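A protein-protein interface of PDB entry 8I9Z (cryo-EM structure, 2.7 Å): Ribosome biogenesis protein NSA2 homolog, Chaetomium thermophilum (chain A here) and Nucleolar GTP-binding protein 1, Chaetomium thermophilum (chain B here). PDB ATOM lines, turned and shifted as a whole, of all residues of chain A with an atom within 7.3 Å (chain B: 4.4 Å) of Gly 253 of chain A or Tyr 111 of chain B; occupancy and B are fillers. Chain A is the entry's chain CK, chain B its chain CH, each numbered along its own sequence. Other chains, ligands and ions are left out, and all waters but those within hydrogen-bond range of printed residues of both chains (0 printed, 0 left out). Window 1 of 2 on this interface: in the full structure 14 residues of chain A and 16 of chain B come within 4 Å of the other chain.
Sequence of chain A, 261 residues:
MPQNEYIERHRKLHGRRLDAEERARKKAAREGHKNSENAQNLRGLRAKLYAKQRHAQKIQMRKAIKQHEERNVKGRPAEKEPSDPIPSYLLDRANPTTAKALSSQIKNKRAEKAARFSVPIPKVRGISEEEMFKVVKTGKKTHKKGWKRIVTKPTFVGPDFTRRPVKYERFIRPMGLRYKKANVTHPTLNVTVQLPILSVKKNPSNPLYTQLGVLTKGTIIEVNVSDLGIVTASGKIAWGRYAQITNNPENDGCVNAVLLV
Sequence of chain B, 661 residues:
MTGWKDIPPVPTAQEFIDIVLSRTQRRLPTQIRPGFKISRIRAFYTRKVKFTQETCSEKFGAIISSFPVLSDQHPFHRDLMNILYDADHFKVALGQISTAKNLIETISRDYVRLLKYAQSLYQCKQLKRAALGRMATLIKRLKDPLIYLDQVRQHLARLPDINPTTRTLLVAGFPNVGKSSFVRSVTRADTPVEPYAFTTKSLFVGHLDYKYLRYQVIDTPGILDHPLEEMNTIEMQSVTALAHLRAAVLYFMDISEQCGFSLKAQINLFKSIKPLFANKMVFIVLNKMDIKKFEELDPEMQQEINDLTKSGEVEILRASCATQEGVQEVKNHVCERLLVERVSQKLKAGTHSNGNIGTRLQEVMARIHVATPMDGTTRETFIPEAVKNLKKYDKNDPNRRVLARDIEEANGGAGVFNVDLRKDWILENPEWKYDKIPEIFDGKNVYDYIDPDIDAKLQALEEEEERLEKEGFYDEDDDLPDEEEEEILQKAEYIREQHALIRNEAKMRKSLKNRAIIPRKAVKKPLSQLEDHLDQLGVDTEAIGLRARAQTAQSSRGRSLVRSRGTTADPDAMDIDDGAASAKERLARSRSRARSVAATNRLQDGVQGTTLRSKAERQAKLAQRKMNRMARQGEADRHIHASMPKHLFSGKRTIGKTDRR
OH of Tyr 111 of chain B is in hydrogen-bond range of N of Gly 253 of chain A (3.0 Å).
The side-chain hydroxyl (OH) of Tyr 179 of chain A lies close to the backbone carbonyl oxygen (O) of Gly 253 of chain A, 3.2 Å away. The side-chain hydroxyl of Tyr 111 of chain B sits close to the guanidinium group of Arg 134 of chain B (3.5 Å).
O of Gly 176 of chain A touches CD2 of Leu 114 of chain B, 3.9 Å away. Tyr 179 of chain A touches Leu 114 of chain B. Leu 127 of chain B touches Asn 251 of chain A (CD2 to O, 3.3 Å). Gly 253 of chain A touches Leu 114 of chain B.
Of chain B, only Tyr 111 (3.0 Å) and Leu 114 (3.7 Å) come within 4 Å of Gly 253 of chain A. Of chain A, only Gly 253 (3.0 Å) comes within 4 Å of Tyr 111 of chain B. Printed residues of chain B within 4 Å of Tyr 179 of chain A: Leu 114. Of the printed residues of chain B, Asn 251 of chain A touches Leu 127. Printed residues of chain A within 4 Å of Leu 127 of chain B: Asn 251. Of the printed residues of chain A, Leu 114 of chain B touches Gly 176, Tyr 179 and Gly 253. The nearest residue of chain A that does not touch Tyr 111 of chain B is Asp 252 of chain A (4.2 Å).
Printed residues of chain B that touch a printed residue of chain A: Tyr 111, Leu 114 and Leu 127. Of the 13 printed residues of chain A, 4 touch a printed residue of chain B. Printed residues of chain A that touch a printed residue of chain B: Gly 176, Tyr 179, Asn 251 and Gly 253.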
ATOM      1  N   GLY A 176       3.512 -11.496 -14.707  1.00  0.00           N
ATOM      2  CA  GLY A 176       4.509 -12.448 -14.256  1.00  0.00           C
ATOM      3  C   GLY A 176       5.761 -12.483 -15.097  1.00  0.00           C
ATOM      4  O   GLY A 176       6.652 -13.294 -14.824  1.00  0.00           O
ATOM      5  N   ARG A 178       7.533  -9.502 -15.974  1.00  0.00           N
ATOM      6  CA  ARG A 178       8.049  -8.146 -15.883  1.00  0.00           C
ATOM      7  C   ARG A 178       9.260  -8.079 -14.964  1.00  0.00           C
ATOM      8  O   ARG A 178       9.450  -8.922 -14.084  1.00  0.00           O
ATOM      9  CB  ARG A 178       6.968  -7.194 -15.373  1.00  0.00           C
ATOM     10  CG  ARG A 178       5.692  -7.234 -16.173  1.00  0.00           C
ATOM     11  CD  ARG A 178       5.109  -5.853 -16.315  1.00  0.00           C
ATOM     12  NE  ARG A 178       3.998  -5.823 -17.255  1.00  0.00           N
ATOM     13  CZ  ARG A 178       2.898  -5.107 -17.086  1.00  0.00           C
ATOM     14  NH1 ARG A 178       2.729  -4.342 -16.021  1.00  0.00           N
ATOM     15  NH2 ARG A 178       1.943  -5.155 -18.008  1.00  0.00           N
ATOM     16  N   TYR A 179      10.080  -7.053 -15.175  1.00  0.00           N
ATOM     17  CA  TYR A 179      11.272  -6.839 -14.371  1.00  0.00           C
ATOM     18  C   TYR A 179      11.425  -5.363 -14.052  1.00  0.00           C
ATOM     19  O   TYR A 179      11.202  -4.506 -14.908  1.00  0.00           O
ATOM     20  CB  TYR A 179      12.529  -7.357 -15.075  1.00  0.00           C
ATOM     21  CG  TYR A 179      12.558  -8.857 -15.205  1.00  0.00           C
ATOM     22  CD1 TYR A 179      13.063  -9.644 -14.185  1.00  0.00           C
ATOM     23  CD2 TYR A 179      12.066  -9.486 -16.334  1.00  0.00           C
ATOM     24  CE1 TYR A 179      13.083 -11.007 -14.288  1.00  0.00           C
ATOM     25  CE2 TYR A 179      12.082 -10.853 -16.444  1.00  0.00           C
ATOM     26  CZ  TYR A 179      12.592 -11.609 -15.418  1.00  0.00           C
ATOM     27  OH  TYR A 179      12.612 -12.978 -15.527  1.00  0.00           O
ATOM     28  N   ASN A 183      20.765  -6.616 -12.322  1.00  0.00           N
ATOM     29  CA  ASN A 183      22.117  -6.792 -11.807  1.00  0.00           C
ATOM     30  C   ASN A 183      23.093  -6.075 -12.730  1.00  0.00           C
ATOM     31  O   ASN A 183      23.323  -6.512 -13.861  1.00  0.00           O
ATOM     32  CB  ASN A 183      22.462  -8.273 -11.691  1.00  0.00           C
ATOM     33  CG  ASN A 183      21.351  -9.078 -11.061  1.00  0.00           C
ATOM     34  OD1 ASN A 183      20.713  -8.634 -10.111  1.00  0.00           O
ATOM     35  ND2 ASN A 183      21.113 -10.270 -11.586  1.00  0.00           N
ATOM     36  N   ASN A 247      23.003 -10.520 -21.128  1.00  0.00           N
ATOM     37  CA  ASN A 247      22.495 -11.873 -20.980  1.00  0.00           C
ATOM     38  C   ASN A 247      21.195 -11.996 -21.759  1.00  0.00           C
ATOM     39  O   ASN A 247      20.721 -11.038 -22.372  1.00  0.00           O
ATOM     40  CB  ASN A 247      22.290 -12.232 -19.504  1.00  0.00           C
ATOM     41  CG  ASN A 247      21.040 -11.618 -18.921  1.00  0.00           C
ATOM     42  OD1 ASN A 247      20.794 -10.424 -19.065  1.00  0.00           O
ATOM     43  ND2 ASN A 247      20.250 -12.432 -18.243  1.00  0.00           N
ATOM     44  N   ASN A 248      20.609 -13.192 -21.730  1.00  0.00           N
ATOM     45  CA  ASN A 248      19.348 -13.479 -22.404  1.00  0.00           C
ATOM     46  C   ASN A 248      18.269 -13.678 -21.354  1.00  0.00           C
ATOM     47  O   ASN A 248      18.074 -14.800 -20.867  1.00  0.00           O
ATOM     48  CB  ASN A 248      19.470 -14.721 -23.288  1.00  0.00           C
ATOM     49  CG  ASN A 248      20.251 -14.461 -24.549  1.00  0.00           C
ATOM     50  OD1 ASN A 248      19.810 -13.714 -25.420  1.00  0.00           O
ATOM     51  ND2 ASN A 248      21.419 -15.078 -24.660  1.00  0.00           N
ATOM     52  N   PRO A 249      17.519 -12.632 -20.989  1.00  0.00           N
ATOM     53  CA  PRO A 249      16.537 -12.768 -19.901  1.00  0.00           C
ATOM     54  C   PRO A 249      15.362 -13.666 -20.239  1.00  0.00           C
ATOM     55  O   PRO A 249      14.558 -13.968 -19.351  1.00  0.00           O
ATOM     56  CB  PRO A 249      16.079 -11.323 -19.662  1.00  0.00           C
ATOM     57  CG  PRO A 249      17.100 -10.469 -20.324  1.00  0.00           C
ATOM     58  CD  PRO A 249      17.584 -11.254 -21.489  1.00  0.00           C
ATOM     59  N   GLU A 250      15.212 -14.072 -21.499  1.00  0.00           N
ATOM     60  CA  GLU A 250      14.222 -15.083 -21.840  1.00  0.00           C
ATOM     61  C   GLU A 250      14.576 -16.425 -21.215  1.00  0.00           C
ATOM     62  O   GLU A 250      13.692 -17.166 -20.772  1.00  0.00           O
ATOM     63  CB  GLU A 250      14.112 -15.208 -23.358  1.00  0.00           C
ATOM     64  CG  GLU A 250      12.714 -15.520 -23.850  1.00  0.00           C
ATOM     65  CD  GLU A 250      12.709 -16.169 -25.218  1.00  0.00           C
ATOM     66  OE1 GLU A 250      13.413 -17.185 -25.397  1.00  0.00           O
ATOM     67  OE2 GLU A 250      11.995 -15.670 -26.114  1.00  0.00           O
ATOM     68  N   ASN A 251      15.866 -16.753 -21.163  1.00  0.00           N
ATOM     69  CA  ASN A 251      16.298 -18.068 -20.710  1.00  0.00           C
ATOM     70  C   ASN A 251      16.549 -18.126 -19.208  1.00  0.00           C
ATOM     71  O   ASN A 251      16.226 -19.134 -18.573  1.00  0.00           O
ATOM     72  CB  ASN A 251      17.555 -18.491 -21.469  1.00  0.00           C
ATOM     73  CG  ASN A 251      17.307 -18.647 -22.949  1.00  0.00           C
ATOM     74  OD1 ASN A 251      16.269 -19.154 -23.362  1.00  0.00           O
ATOM     75  ND2 ASN A 251      18.264 -18.221 -23.758  1.00  0.00           N
ATOM     76  N   ASP A 252      17.125 -17.083 -18.619  1.00  0.00           N
ATOM     77  CA  ASP A 252      17.279 -17.016 -17.174  1.00  0.00           C
ATOM     78  C   ASP A 252      16.397 -15.916 -16.597  1.00  0.00           C
ATOM     79  O   ASP A 252      16.154 -14.889 -17.234  1.00  0.00           O
ATOM     80  CB  ASP A 252      18.748 -16.820 -16.769  1.00  0.00           C
ATOM     81  CG  ASP A 252      19.414 -15.628 -17.441  1.00  0.00           C
ATOM     82  OD1 ASP A 252      18.759 -14.867 -18.175  1.00  0.00           O
ATOM     83  OD2 ASP A 252      20.630 -15.451 -17.235  1.00  0.00           O
ATOM     84  N   GLY A 253      15.908 -16.141 -15.388  1.00  0.00           N
ATOM     85  CA  GLY A 253      14.933 -15.245 -14.804  1.00  0.00           C
ATOM     86  C   GLY A 253      15.468 -13.963 -14.216  1.00  0.00           C
ATOM     87  O   GLY A 253      14.875 -13.435 -13.273  1.00  0.00           O
ATOM     88  N   CYS A 254      16.571 -13.445 -14.734  1.00  0.00           N
ATOM     89  CA  CYS A 254      17.191 -12.224 -14.249  1.00  0.00           C
ATOM     90  C   CYS A 254      17.629 -11.370 -15.433  1.00  0.00           C
ATOM     91  O   CYS A 254      17.649 -11.818 -16.580  1.00  0.00           O
ATOM     92  CB  CYS A 254      18.381 -12.543 -13.340  1.00  0.00           C
ATOM     93  SG  CYS A 254      19.550 -13.731 -14.030  1.00  0.00           S
ATOM     94  N   VAL A 255      17.986 -10.125 -15.137  1.00  0.00           N
ATOM     95  CA  VAL A 255      18.508  -9.189 -16.120  1.00  0.00           C
ATOM     96  C   VAL A 255      19.908  -8.800 -15.675  1.00  0.00           C
ATOM     97  O   VAL A 255      20.092  -8.297 -14.561  1.00  0.00           O
ATOM     98  CB  VAL A 255      17.610  -7.951 -16.265  1.00  0.00           C
ATOM     99  CG1 VAL A 255      18.281  -6.907 -17.126  1.00  0.00           C
ATOM    100  CG2 VAL A 255      16.272  -8.340 -16.855  1.00  0.00           C
ATOM    101  N   ILE B 107      11.712 -17.988  -5.465  1.00  0.00           N
ATOM    102  CA  ILE B 107      12.301 -18.374  -6.746  1.00  0.00           C
ATOM    103  C   ILE B 107      11.393 -19.355  -7.474  1.00  0.00           C
ATOM    104  O   ILE B 107      11.172 -19.238  -8.686  1.00  0.00           O
ATOM    105  CB  ILE B 107      13.712 -18.951  -6.526  1.00  0.00           C
ATOM    106  CG1 ILE B 107      14.699 -17.836  -6.202  1.00  0.00           C
ATOM    107  CG2 ILE B 107      14.198 -19.716  -7.740  1.00  0.00           C
ATOM    108  CD1 ILE B 107      16.067 -18.336  -5.829  1.00  0.00           C
ATOM    109  N   SER B 108      10.840 -20.322  -6.743  1.00  0.00           N
ATOM    110  CA  SER B 108       9.942 -21.298  -7.347  1.00  0.00           C
ATOM    111  C   SER B 108       8.668 -20.639  -7.858  1.00  0.00           C
ATOM    112  O   SER B 108       8.133 -21.026  -8.901  1.00  0.00           O
ATOM    113  CB  SER B 108       9.612 -22.390  -6.334  1.00  0.00           C
ATOM    114  OG  SER B 108       8.520 -23.174  -6.772  1.00  0.00           O
ATOM    115  N   ARG B 109       8.166 -19.640  -7.133  1.00  0.00           N
ATOM    116  CA  ARG B 109       6.956 -18.946  -7.558  1.00  0.00           C
ATOM    117  C   ARG B 109       7.208 -18.119  -8.812  1.00  0.00           C
ATOM    118  O   ARG B 109       6.338 -18.007  -9.682  1.00  0.00           O
ATOM    119  CB  ARG B 109       6.441 -18.067  -6.420  1.00  0.00           C
ATOM    120  CG  ARG B 109       5.108 -17.404  -6.692  1.00  0.00           C
ATOM    121  CD  ARG B 109       4.478 -16.750  -5.452  1.00  0.00           C
ATOM    122  NE  ARG B 109       5.419 -16.098  -4.546  1.00  0.00           N
ATOM    123  CZ  ARG B 109       5.883 -16.629  -3.420  1.00  0.00           C
ATOM    124  NH1 ARG B 109       5.534 -17.845  -3.035  1.00  0.00           N
ATOM    125  NH2 ARG B 109       6.723 -15.925  -2.667  1.00  0.00           N
ATOM    126  N   ASP B 110       8.402 -17.538  -8.924  1.00  0.00           N
ATOM    127  CA  ASP B 110       8.716 -16.709 -10.081  1.00  0.00           C
ATOM    128  C   ASP B 110       8.934 -17.553 -11.330  1.00  0.00           C
ATOM    129  O   ASP B 110       8.436 -17.222 -12.411  1.00  0.00           O
ATOM    130  CB  ASP B 110       9.948 -15.853  -9.790  1.00  0.00           C
ATOM    131  CG  ASP B 110       9.631 -14.650  -8.925  1.00  0.00           C
ATOM    132  OD1 ASP B 110      10.580 -13.953  -8.509  1.00  0.00           O
ATOM    133  OD2 ASP B 110       8.437 -14.398  -8.661  1.00  0.00           O
ATOM    134  N   TYR B 111       9.680 -18.651 -11.203  1.00  0.00           N
ATOM    135  CA  TYR B 111      10.065 -19.421 -12.381  1.00  0.00           C
ATOM    136  C   TYR B 111       8.950 -20.325 -12.891  1.00  0.00           C
ATOM    137  O   TYR B 111       8.976 -20.720 -14.060  1.00  0.00           O
ATOM    138  CB  TYR B 111      11.316 -20.241 -12.089  1.00  0.00           C
ATOM    139  CG  TYR B 111      12.600 -19.462 -12.234  1.00  0.00           C
ATOM    140  CD1 TYR B 111      13.262 -19.396 -13.448  1.00  0.00           C
ATOM    141  CD2 TYR B 111      13.154 -18.800 -11.153  1.00  0.00           C
ATOM    142  CE1 TYR B 111      14.435 -18.689 -13.578  1.00  0.00           C
ATOM    143  CE2 TYR B 111      14.325 -18.095 -11.275  1.00  0.00           C
ATOM    144  CZ  TYR B 111      14.958 -18.041 -12.488  1.00  0.00           C
ATOM    145  OH  TYR B 111      16.129 -17.335 -12.601  1.00  0.00           O
ATOM    146  N   VAL B 112       7.981 -20.674 -12.045  1.00  0.00           N
ATOM    147  CA  VAL B 112       6.799 -21.384 -12.526  1.00  0.00           C
ATOM    148  C   VAL B 112       5.981 -20.473 -13.433  1.00  0.00           C
ATOM    149  O   VAL B 112       5.452 -20.906 -14.465  1.00  0.00           O
ATOM    150  CB  VAL B 112       5.980 -21.920 -11.334  1.00  0.00           C
ATOM    151  CG1 VAL B 112       4.532 -22.184 -11.711  1.00  0.00           C
ATOM    152  CG2 VAL B 112       6.607 -23.189 -10.800  1.00  0.00           C
ATOM    153  N   ARG B 113       5.904 -19.189 -13.084  1.00  0.00           N
ATOM    154  CA  ARG B 113       5.241 -18.211 -13.939  1.00  0.00           C
ATOM    155  C   ARG B 113       5.977 -18.039 -15.262  1.00  0.00           C
ATOM    156  O   ARG B 113       5.353 -17.876 -16.314  1.00  0.00           O
ATOM    157  CB  ARG B 113       5.139 -16.871 -13.220  1.00  0.00           C
ATOM    158  CG  ARG B 113       4.227 -16.879 -12.031  1.00  0.00           C
ATOM    159  CD  ARG B 113       3.878 -15.468 -11.628  1.00  0.00           C
ATOM    160  NE  ARG B 113       2.891 -15.445 -10.558  1.00  0.00           N
ATOM    161  CZ  ARG B 113       3.138 -15.022  -9.327  1.00  0.00           C
ATOM    162  NH1 ARG B 113       4.334 -14.579  -8.978  1.00  0.00           N
ATOM    163  NH2 ARG B 113       2.163 -15.047  -8.424  1.00  0.00           N
ATOM    164  N   LEU B 114       7.309 -18.047 -15.220  1.00  0.00           N
ATOM    165  CA  LEU B 114       8.091 -17.898 -16.442  1.00  0.00           C
ATOM    166  C   LEU B 114       7.923 -19.106 -17.351  1.00  0.00           C
ATOM    167  O   LEU B 114       7.922 -18.972 -18.579  1.00  0.00           O
ATOM    168  CB  LEU B 114       9.563 -17.686 -16.099  1.00  0.00           C
ATOM    169  CG  LEU B 114       9.934 -16.368 -15.426  1.00  0.00           C
ATOM    170  CD1 LEU B 114      11.380 -16.390 -14.993  1.00  0.00           C
ATOM    171  CD2 LEU B 114       9.676 -15.205 -16.353  1.00  0.00           C
ATOM    172  N   LEU B 115       7.773 -20.295 -16.762  1.00  0.00           N
ATOM    173  CA  LEU B 115       7.593 -21.504 -17.556  1.00  0.00           C
ATOM    174  C   LEU B 115       6.228 -21.530 -18.227  1.00  0.00           C
ATOM    175  O   LEU B 115       6.026 -22.252 -19.209  1.00  0.00           O
ATOM    176  CB  LEU B 115       7.780 -22.737 -16.674  1.00  0.00           C
ATOM    177  CG  LEU B 115       9.215 -23.201 -16.458  1.00  0.00           C
ATOM    178  CD1 LEU B 115       9.309 -24.101 -15.247  1.00  0.00           C
ATOM    179  CD2 LEU B 115       9.716 -23.911 -17.693  1.00  0.00           C
ATOM    180  N   LEU B 127      15.166 -22.460 -18.112  1.00  0.00           N
ATOM    181  CA  LEU B 127      14.446 -21.911 -16.968  1.00  0.00           C
ATOM    182  C   LEU B 127      14.418 -22.895 -15.807  1.00  0.00           C
ATOM    183  O   LEU B 127      14.435 -22.482 -14.641  1.00  0.00           O
ATOM    184  CB  LEU B 127      13.030 -21.516 -17.373  1.00  0.00           C
ATOM    185  CG  LEU B 127      12.882 -20.174 -18.088  1.00  0.00           C
ATOM    186  CD1 LEU B 127      11.485 -20.027 -18.645  1.00  0.00           C
ATOM    187  CD2 LEU B 127      13.201 -19.030 -17.149  1.00  0.00           C
ATOM    188  N   ALA B 130      18.053 -22.732 -14.360  1.00  0.00           N
ATOM    189  CA  ALA B 130      18.311 -21.489 -13.647  1.00  0.00           C
ATOM    190  C   ALA B 130      17.684 -21.511 -12.261  1.00  0.00           C
ATOM    191  O   ALA B 130      18.291 -21.064 -11.283  1.00  0.00           O
ATOM    192  CB  ALA B 130      17.789 -20.304 -14.460  1.00  0.00           C
ATOM    193  N   ALA B 131      16.463 -22.033 -12.163  1.00  0.00           N
ATOM    194  CA  ALA B 131      15.779 -22.115 -10.878  1.00  0.00           C
ATOM    195  C   ALA B 131      16.477 -23.088  -9.940  1.00  0.00           C
ATOM    196  O   ALA B 131      16.583 -22.844  -8.734  1.00  0.00           O
ATOM    197  CB  ALA B 131      14.324 -22.530 -11.095  1.00  0.00           C
ATOM    198  N   ARG B 134      19.877 -21.540  -8.855  1.00  0.00           N
ATOM    199  CA  ARG B 134      19.700 -20.455  -7.897  1.00  0.00           C
ATOM    200  C   ARG B 134      19.327 -20.990  -6.524  1.00  0.00           C
ATOM    201  O   ARG B 134      19.747 -20.437  -5.503  1.00  0.00           O
ATOM    202  CB  ARG B 134      18.649 -19.468  -8.396  1.00  0.00           C
ATOM    203  CG  ARG B 134      19.178 -18.526  -9.445  1.00  0.00           C
ATOM    204  CD  ARG B 134      18.171 -17.482  -9.846  1.00  0.00           C
ATOM    205  NE  ARG B 134      17.762 -16.669  -8.712  1.00  0.00           N
ATOM    206  CZ  ARG B 134      17.042 -15.562  -8.813  1.00  0.00           C
ATOM    207  NH1 ARG B 134      16.648 -15.102  -9.987  1.00  0.00           N
ATOM    208  NH2 ARG B 134      16.708 -14.902  -7.710  1.00  0.00           N
